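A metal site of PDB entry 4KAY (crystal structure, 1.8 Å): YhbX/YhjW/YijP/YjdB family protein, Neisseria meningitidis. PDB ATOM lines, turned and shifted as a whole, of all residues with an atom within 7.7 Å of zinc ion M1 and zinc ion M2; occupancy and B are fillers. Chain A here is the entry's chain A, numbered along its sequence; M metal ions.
Of the 27 residues printed, 3 come within 4 Å of zinc ion M1. The nearest printed residue that does not touch zinc ion M1 is Glu 31 (4.5 Å).
Zinc ion M2 is bound by the side-chain carboxylate (OE2) of Glu 31, the side-chain carboxylate (OD2) of Asp 243, OG1 of TPO 71, a ring nitrogen (NE2) of His 244 and the side-chain carboxylate (OE1) of Glu 31.
O2P of TPO 71 is bound to zinc ion M1. Zinc ion M1 is bound by NE2 of His 174. NE2 of His 256 is bound to zinc ion M1 (2.3 Å). O3P of TPO 71 binds zinc ion M1 (2.5 Å). Zinc ion M1 has four donor atoms within binding distance.
The side-chain carboxylate (OE2) of Glu 31 sits close to the side-chain hydroxyl (OG1) of Thr 32 (2.8 Å). OE1 of Glu 31 lies close to OD2 of Asp 115 (2.6 Å). The backbone NH (N) of Thr 32 sits at hydrogen-bond distance from the side-chain carboxylate (OD1) of Asp 243, at 3.0 Å. The backbone NH of Asp 243 sits at hydrogen-bond distance from the backbone carbonyl oxygen of Gly 30, at 3.4 Å. The side-chain hydroxyl (OG) of Ser 74 sits at hydrogen-bond distance from the backbone carbonyl oxygen (O) of Asp 243 (2.7 Å). N of Thr 32 lies close to O of His 244 (3.3 Å). The side-chain hydroxyl (OG) of Ser 242 lies within hydrogen-bond range of the backbone carbonyl oxygen (O) of His 244 (3.0 Å). ND1 of His 256 lies within hydrogen-bond range of OE1 of Glu 246, 2.7 Å away.
Four residues have an atom within 4 Å of zinc ion M2: Glu 31, TPO 71, Asp 243 and His 244. The nearest printed residue that does not touch zinc ion M2 is Thr 32 (4.3 Å).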
ATOM      1  N   GLY A  30     -21.209  17.949 -31.827  1.00  0.00           N
ATOM      2  CA  GLY A  30     -20.298  17.831 -30.697  1.00  0.00           C
ATOM      3  C   GLY A  30     -20.070  16.387 -30.309  1.00  0.00           C
ATOM      4  O   GLY A  30     -20.676  15.454 -30.851  1.00  0.00           O
ATOM      5  N   GLU A  31     -19.157  16.208 -29.358  1.00  0.00           N
ATOM      6  CA  GLU A  31     -18.770  14.893 -28.899  1.00  0.00           C
ATOM      7  C   GLU A  31     -18.368  14.892 -27.431  1.00  0.00           C
ATOM      8  O   GLU A  31     -17.332  15.456 -27.055  1.00  0.00           O
ATOM      9  CB  GLU A  31     -17.620  14.355 -29.752  1.00  0.00           C
ATOM     10  CG  GLU A  31     -17.041  13.045 -29.254  1.00  0.00           C
ATOM     11  CD  GLU A  31     -18.046  11.915 -29.279  1.00  0.00           C
ATOM     12  OE1 GLU A  31     -18.326  11.391 -30.387  1.00  0.00           O
ATOM     13  OE2 GLU A  31     -18.547  11.534 -28.207  1.00  0.00           O
ATOM     14  N   THR A  32     -19.193  14.253 -26.606  1.00  0.00           N
ATOM     15  CA  THR A  32     -18.874  13.978 -25.194  1.00  0.00           C
ATOM     16  C   THR A  32     -19.062  15.195 -24.289  1.00  0.00           C
ATOM     17  O   THR A  32     -19.114  15.072 -23.162  1.00  0.00           O
ATOM     18  CB  THR A  32     -17.452  13.393 -25.028  1.00  0.00           C
ATOM     19  OG1 THR A  32     -17.342  12.223 -25.792  1.00  0.00           O
ATOM     20  CG2 THR A  32     -17.154  13.046 -23.593  1.00  0.00           C
ATOM     21  N   THR A  33     -19.180  16.358 -24.854  1.00  0.00           N
ATOM     22  CA  THR A  33     -19.358  17.565 -24.072  1.00  0.00           C
ATOM     23  C   THR A  33     -20.699  17.546 -23.368  1.00  0.00           C
ATOM     24  O   THR A  33     -21.670  17.307 -24.001  1.00  0.00           O
ATOM     25  CB  THR A  33     -19.246  18.825 -24.963  1.00  0.00           C
ATOM     26  OG1 THR A  33     -18.069  18.762 -25.739  1.00  0.00           O
ATOM     27  CG2 THR A  33     -19.189  20.034 -24.154  1.00  0.00           C
ATOM     28  N   THR A  69     -26.174   7.271 -25.121  1.00  0.00           N
ATOM     29  CA  THR A  69     -24.994   7.651 -24.307  1.00  0.00           C
ATOM     30  C   THR A  69     -23.715   7.252 -25.021  1.00  0.00           C
ATOM     31  O   THR A  69     -22.591   7.305 -24.466  1.00  0.00           O
ATOM     32  CB  THR A  69     -25.049   6.956 -22.940  1.00  0.00           C
ATOM     33  OG1 THR A  69     -25.230   5.558 -23.150  1.00  0.00           O
ATOM     34  CG2 THR A  69     -26.205   7.507 -22.106  1.00  0.00           C
ATOM     35  N   SER A  70     -23.848   6.839 -26.274  1.00  0.00           N
ATOM     36  CA  SER A  70     -22.716   6.595 -27.101  1.00  0.00           C
ATOM     37  C   SER A  70     -22.947   7.126 -28.501  1.00  0.00           C
ATOM     38  O   SER A  70     -24.083   7.282 -28.947  1.00  0.00           O
ATOM     39  CB  SER A  70     -22.416   5.104 -27.182  1.00  0.00           C
ATOM     40  OG  SER A  70     -23.461   4.467 -27.900  1.00  0.00           O
ATOM     41  N   TPO A  71     -21.849   7.343 -29.204  1.00  0.00           N
ATOM     42  CA  TPO A  71     -21.851   7.939 -30.519  1.00  0.00           C
ATOM     43  CB  TPO A  71     -20.429   8.132 -30.998  1.00  0.00           C
ATOM     44  CG2 TPO A  71     -20.370   9.141 -32.146  1.00  0.00           C
ATOM     45  OG1 TPO A  71     -19.705   8.664 -29.889  1.00  0.00           O
ATOM     46  P   TPO A  71     -18.529   7.600 -29.422  1.00  0.00           P
ATOM     47  O1P TPO A  71     -17.889   6.855 -30.534  1.00  0.00           O
ATOM     48  O2P TPO A  71     -17.482   8.625 -28.784  1.00  0.00           O
ATOM     49  O3P TPO A  71     -19.043   6.568 -28.283  1.00  0.00           O
ATOM     50  C   TPO A  71     -22.628   7.079 -31.501  1.00  0.00           C
ATOM     51  O   TPO A  71     -23.375   7.592 -32.282  1.00  0.00           O
ATOM     52  N   ALA A  72     -22.381   5.775 -31.485  1.00  0.00           N
ATOM     53  CA  ALA A  72     -22.947   4.911 -32.502  1.00  0.00           C
ATOM     54  C   ALA A  72     -24.451   4.836 -32.331  1.00  0.00           C
ATOM     55  O   ALA A  72     -25.150   4.427 -33.279  1.00  0.00           O
ATOM     56  CB  ALA A  72     -22.316   3.516 -32.446  1.00  0.00           C
ATOM     57  N   HIS A  73     -24.961   5.157 -31.140  1.00  0.00           N
ATOM     58  CA  HIS A  73     -26.402   5.234 -30.909  1.00  0.00           C
ATOM     59  C   HIS A  73     -26.927   6.638 -31.245  1.00  0.00           C
ATOM     60  O   HIS A  73     -27.848   6.791 -32.062  1.00  0.00           O
ATOM     61  CB  HIS A  73     -26.742   4.890 -29.456  1.00  0.00           C
ATOM     62  CG  HIS A  73     -28.219   4.760 -29.193  1.00  0.00           C
ATOM     63  ND1 HIS A  73     -28.850   3.543 -29.106  1.00  0.00           N
ATOM     64  CD2 HIS A  73     -29.184   5.698 -29.058  1.00  0.00           C
ATOM     65  CE1 HIS A  73     -30.135   3.728 -28.885  1.00  0.00           C
ATOM     66  NE2 HIS A  73     -30.368   5.021 -28.846  1.00  0.00           N
ATOM     67  N   SER A  74     -26.368   7.659 -30.611  1.00  0.00           N
ATOM     68  CA  SER A  74     -26.891   9.012 -30.802  1.00  0.00           C
ATOM     69  C   SER A  74     -26.869   9.545 -32.226  1.00  0.00           C
ATOM     70  O   SER A  74     -27.834  10.224 -32.654  1.00  0.00           O
ATOM     71  CB  SER A  74     -26.168   9.988 -29.881  1.00  0.00           C
ATOM     72  OG  SER A  74     -26.496   9.743 -28.533  1.00  0.00           O
ATOM     73  N   LEU A  75     -25.800   9.314 -32.981  1.00  0.00           N
ATOM     74  CA  LEU A  75     -25.692   9.945 -34.281  1.00  0.00           C
ATOM     75  C   LEU A  75     -26.760   9.383 -35.218  1.00  0.00           C
ATOM     76  O   LEU A  75     -27.503  10.118 -35.855  1.00  0.00           O
ATOM     77  CB  LEU A  75     -24.331   9.760 -34.924  1.00  0.00           C
ATOM     78  CG  LEU A  75     -23.583  11.073 -35.127  1.00  0.00           C
ATOM     79  CD1 LEU A  75     -23.217  11.623 -33.760  1.00  0.00           C
ATOM     80  CD2 LEU A  75     -22.333  10.810 -35.974  1.00  0.00           C
ATOM     81  N   ASP A 115     -14.017  12.751 -36.167  1.00  0.00           N
ATOM     82  CA  ASP A 115     -14.350  12.018 -34.928  1.00  0.00           C
ATOM     83  C   ASP A 115     -14.384  10.468 -35.097  1.00  0.00           C
ATOM     84  O   ASP A 115     -15.133   9.741 -34.410  1.00  0.00           O
ATOM     85  CB  ASP A 115     -15.685  12.540 -34.388  1.00  0.00           C
ATOM     86  CG  ASP A 115     -16.043  12.024 -33.009  1.00  0.00           C
ATOM     87  OD1 ASP A 115     -15.146  11.841 -32.142  1.00  0.00           O
ATOM     88  OD2 ASP A 115     -17.266  11.807 -32.765  1.00  0.00           O
ATOM     89  N   SER A 116     -13.547   9.981 -35.993  1.00  0.00           N
ATOM     90  CA  SER A 116     -13.330   8.528 -36.212  1.00  0.00           C
ATOM     91  C   SER A 116     -14.413   7.827 -37.055  1.00  0.00           C
ATOM     92  O   SER A 116     -14.238   6.656 -37.418  1.00  0.00           O
ATOM     93  CB  SER A 116     -13.154   7.738 -34.899  1.00  0.00           C
ATOM     94  OG  SER A 116     -14.381   7.232 -34.393  1.00  0.00           O
ATOM     95  N   LYS A 119     -20.684   7.023 -38.707  1.00  0.00           N
ATOM     96  CA  LYS A 119     -21.622   6.023 -38.203  1.00  0.00           C
ATOM     97  C   LYS A 119     -22.748   5.733 -39.198  1.00  0.00           C
ATOM     98  O   LYS A 119     -23.936   5.624 -38.817  1.00  0.00           O
ATOM     99  CB  LYS A 119     -22.243   6.472 -36.881  1.00  0.00           C
ATOM    100  CG  LYS A 119     -21.235   6.839 -35.809  1.00  0.00           C
ATOM    101  CD  LYS A 119     -20.253   5.702 -35.553  1.00  0.00           C
ATOM    102  CE  LYS A 119     -19.523   5.877 -34.211  1.00  0.00           C
ATOM    103  NZ  LYS A 119     -18.482   4.840 -34.007  1.00  0.00           N
ATOM    104  N   HIS A 169     -18.312  17.406 -37.918  1.00  0.00           N
ATOM    105  CA  HIS A 169     -18.416  16.424 -36.856  1.00  0.00           C
ATOM    106  C   HIS A 169     -17.129  16.407 -36.066  1.00  0.00           C
ATOM    107  O   HIS A 169     -16.087  15.945 -36.558  1.00  0.00           O
ATOM    108  CB  HIS A 169     -18.680  15.012 -37.431  1.00  0.00           C
ATOM    109  CG  HIS A 169     -18.913  13.980 -36.362  1.00  0.00           C
ATOM    110  ND1 HIS A 169     -18.740  12.624 -36.580  1.00  0.00           N
ATOM    111  CD2 HIS A 169     -19.306  14.106 -35.068  1.00  0.00           C
ATOM    112  CE1 HIS A 169     -19.017  11.971 -35.473  1.00  0.00           C
ATOM    113  NE2 HIS A 169     -19.383  12.845 -34.545  1.00  0.00           N
ATOM    114  N   THR A 170     -17.193  16.956 -34.866  1.00  0.00           N
ATOM    115  CA  THR A 170     -16.015  17.149 -34.043  1.00  0.00           C
ATOM    116  C   THR A 170     -15.689  16.017 -33.081  1.00  0.00           C
ATOM    117  O   THR A 170     -16.548  15.167 -32.775  1.00  0.00           O
ATOM    118  CB  THR A 170     -16.240  18.419 -33.208  1.00  0.00           C
ATOM    119  OG1 THR A 170     -17.358  18.199 -32.324  1.00  0.00           O
ATOM    120  CG2 THR A 170     -16.508  19.588 -34.122  1.00  0.00           C
ATOM    121  N   ILE A 171     -14.433  16.025 -32.578  1.00  0.00           N
ATOM    122  CA  ILE A 171     -14.003  15.117 -31.523  1.00  0.00           C
ATOM    123  C   ILE A 171     -14.207  15.700 -30.134  1.00  0.00           C
ATOM    124  O   ILE A 171     -14.323  14.968 -29.130  1.00  0.00           O
ATOM    125  CB  ILE A 171     -12.547  14.594 -31.768  1.00  0.00           C
ATOM    126  CG1 ILE A 171     -12.257  13.460 -30.795  1.00  0.00           C
ATOM    127  CG2 ILE A 171     -11.510  15.699 -31.663  1.00  0.00           C
ATOM    128  CD1 ILE A 171     -11.065  12.596 -31.251  1.00  0.00           C
ATOM    129  N   HIS A 174     -13.842  14.204 -26.236  1.00  0.00           N
ATOM    130  CA  HIS A 174     -13.674  12.762 -26.141  1.00  0.00           C
ATOM    131  C   HIS A 174     -12.432  12.417 -25.325  1.00  0.00           C
ATOM    132  O   HIS A 174     -11.378  13.018 -25.497  1.00  0.00           O
ATOM    133  CB  HIS A 174     -13.585  12.127 -27.503  1.00  0.00           C
ATOM    134  CG  HIS A 174     -14.074  10.717 -27.536  1.00  0.00           C
ATOM    135  ND1 HIS A 174     -13.348   9.657 -27.018  1.00  0.00           N
ATOM    136  CD2 HIS A 174     -15.226  10.167 -28.013  1.00  0.00           C
ATOM    137  CE1 HIS A 174     -14.029   8.535 -27.173  1.00  0.00           C
ATOM    138  NE2 HIS A 174     -15.178   8.817 -27.769  1.00  0.00           N
ATOM    139  N   GLY A 175     -12.594  11.447 -24.442  1.00  0.00           N
ATOM    140  CA  GLY A 175     -11.500  10.904 -23.640  1.00  0.00           C
ATOM    141  C   GLY A 175     -11.170   9.467 -24.053  1.00  0.00           C
ATOM    142  O   GLY A 175     -11.744   8.922 -25.013  1.00  0.00           O
ATOM    143  N   SER A 242     -24.167  18.493 -28.651  1.00  0.00           N
ATOM    144  CA  SER A 242     -23.316  17.325 -28.399  1.00  0.00           C
ATOM    145  C   SER A 242     -24.070  16.009 -28.660  1.00  0.00           C
ATOM    146  O   SER A 242     -25.305  15.993 -28.716  1.00  0.00           O
ATOM    147  CB  SER A 242     -22.817  17.311 -26.955  1.00  0.00           C
ATOM    148  OG  SER A 242     -21.786  16.351 -26.828  1.00  0.00           O
ATOM    149  N   ASP A 243     -23.324  14.923 -28.855  1.00  0.00           N
ATOM    150  CA  ASP A 243     -23.965  13.604 -29.006  1.00  0.00           C
ATOM    151  C   ASP A 243     -24.384  12.910 -27.711  1.00  0.00           C
ATOM    152  O   ASP A 243     -25.296  12.075 -27.713  1.00  0.00           O
ATOM    153  CB  ASP A 243     -23.109  12.667 -29.873  1.00  0.00           C
ATOM    154  CG  ASP A 243     -21.819  12.271 -29.217  1.00  0.00           C
ATOM    155  OD1 ASP A 243     -21.298  13.009 -28.331  1.00  0.00           O
ATOM    156  OD2 ASP A 243     -21.275  11.256 -29.677  1.00  0.00           O
ATOM    157  N   HIS A 244     -23.731  13.267 -26.614  1.00  0.00           N
ATOM    158  CA  HIS A 244     -23.962  12.702 -25.295  1.00  0.00           C
ATOM    159  C   HIS A 244     -22.939  13.356 -24.408  1.00  0.00           C
ATOM    160  O   HIS A 244     -22.014  14.007 -24.906  1.00  0.00           O
ATOM    161  CB  HIS A 244     -23.728  11.175 -25.266  1.00  0.00           C
ATOM    162  CG  HIS A 244     -22.372  10.742 -25.813  1.00  0.00           C
ATOM    163  ND1 HIS A 244     -21.186  10.866 -25.098  1.00  0.00           N
ATOM    164  CD2 HIS A 244     -22.044  10.185 -26.996  1.00  0.00           C
ATOM    165  CE1 HIS A 244     -20.189  10.436 -25.847  1.00  0.00           C
ATOM    166  NE2 HIS A 244     -20.675  10.019 -27.009  1.00  0.00           N
ATOM    167  N   GLY A 245     -23.079  13.132 -23.112  1.00  0.00           N
ATOM    168  CA  GLY A 245     -22.165  13.632 -22.117  1.00  0.00           C
ATOM    169  C   GLY A 245     -21.093  12.641 -21.689  1.00  0.00           C
ATOM    170  O   GLY A 245     -20.680  11.778 -22.449  1.00  0.00           O
ATOM    171  N   GLU A 246     -20.662  12.810 -20.441  1.00  0.00           N
ATOM    172  CA  GLU A 246     -19.532  12.066 -19.935  1.00  0.00           C
ATOM    173  C   GLU A 246     -19.686  11.988 -18.429  1.00  0.00           C
ATOM    174  O   GLU A 246     -20.239  12.890 -17.787  1.00  0.00           O
ATOM    175  CB  GLU A 246     -18.241  12.871 -20.237  1.00  0.00           C
ATOM    176  CG  GLU A 246     -16.911  12.088 -19.968  1.00  0.00           C
ATOM    177  CD  GLU A 246     -16.617  11.027 -21.010  1.00  0.00           C
ATOM    178  OE1 GLU A 246     -17.562  10.470 -21.600  1.00  0.00           O
ATOM    179  OE2 GLU A 246     -15.422  10.716 -21.264  1.00  0.00           O
ATOM    180  N   LEU A 255     -16.087   7.853 -18.270  1.00  0.00           N
ATOM    181  CA  LEU A 255     -16.368   7.736 -19.706  1.00  0.00           C
ATOM    182  C   LEU A 255     -17.878   7.802 -19.919  1.00  0.00           C
ATOM    183  O   LEU A 255     -18.532   8.480 -19.206  1.00  0.00           O
ATOM    184  CB  LEU A 255     -15.706   6.466 -20.255  1.00  0.00           C
ATOM    185  CG  LEU A 255     -14.246   6.233 -19.962  1.00  0.00           C
ATOM    186  CD1 LEU A 255     -13.755   4.918 -20.549  1.00  0.00           C
ATOM    187  CD2 LEU A 255     -13.442   7.354 -20.519  1.00  0.00           C
ATOM    188  N   HIS A 256     -18.369   7.171 -20.983  1.00  0.00           N
ATOM    189  CA  HIS A 256     -19.780   7.207 -21.280  1.00  0.00           C
ATOM    190  C   HIS A 256     -20.360   5.801 -21.589  1.00  0.00           C
ATOM    191  O   HIS A 256     -19.924   4.842 -21.026  1.00  0.00           O
ATOM    192  CB  HIS A 256     -20.000   8.290 -22.358  1.00  0.00           C
ATOM    193  CG  HIS A 256     -19.146   8.139 -23.555  1.00  0.00           C
ATOM    194  ND1 HIS A 256     -17.963   8.812 -23.682  1.00  0.00           N
ATOM    195  CD2 HIS A 256     -19.300   7.454 -24.714  1.00  0.00           C
ATOM    196  CE1 HIS A 256     -17.431   8.536 -24.848  1.00  0.00           C
ATOM    197  NE2 HIS A 256     -18.217   7.702 -25.483  1.00  0.00           N
ATOM    198  N   ALA A 257     -21.349   5.738 -22.458  1.00  0.00           N
ATOM    199  CA  ALA A 257     -21.976   4.462 -22.842  1.00  0.00           C
ATOM    200  C   ALA A 257     -22.664   3.708 -21.678  1.00  0.00           C
ATOM    201  O   ALA A 257     -22.916   2.542 -21.786  1.00  0.00           O
ATOM    202  CB  ALA A 257     -20.940   3.574 -23.485  1.00  0.00           C
HETATM  203 ZN    ZN M   1     -16.862   7.436 -27.363  1.00  0.00          ZN
HETATM  204 ZN    ZN M   2     -19.796  10.302 -28.777  1.00  0.00          ZN
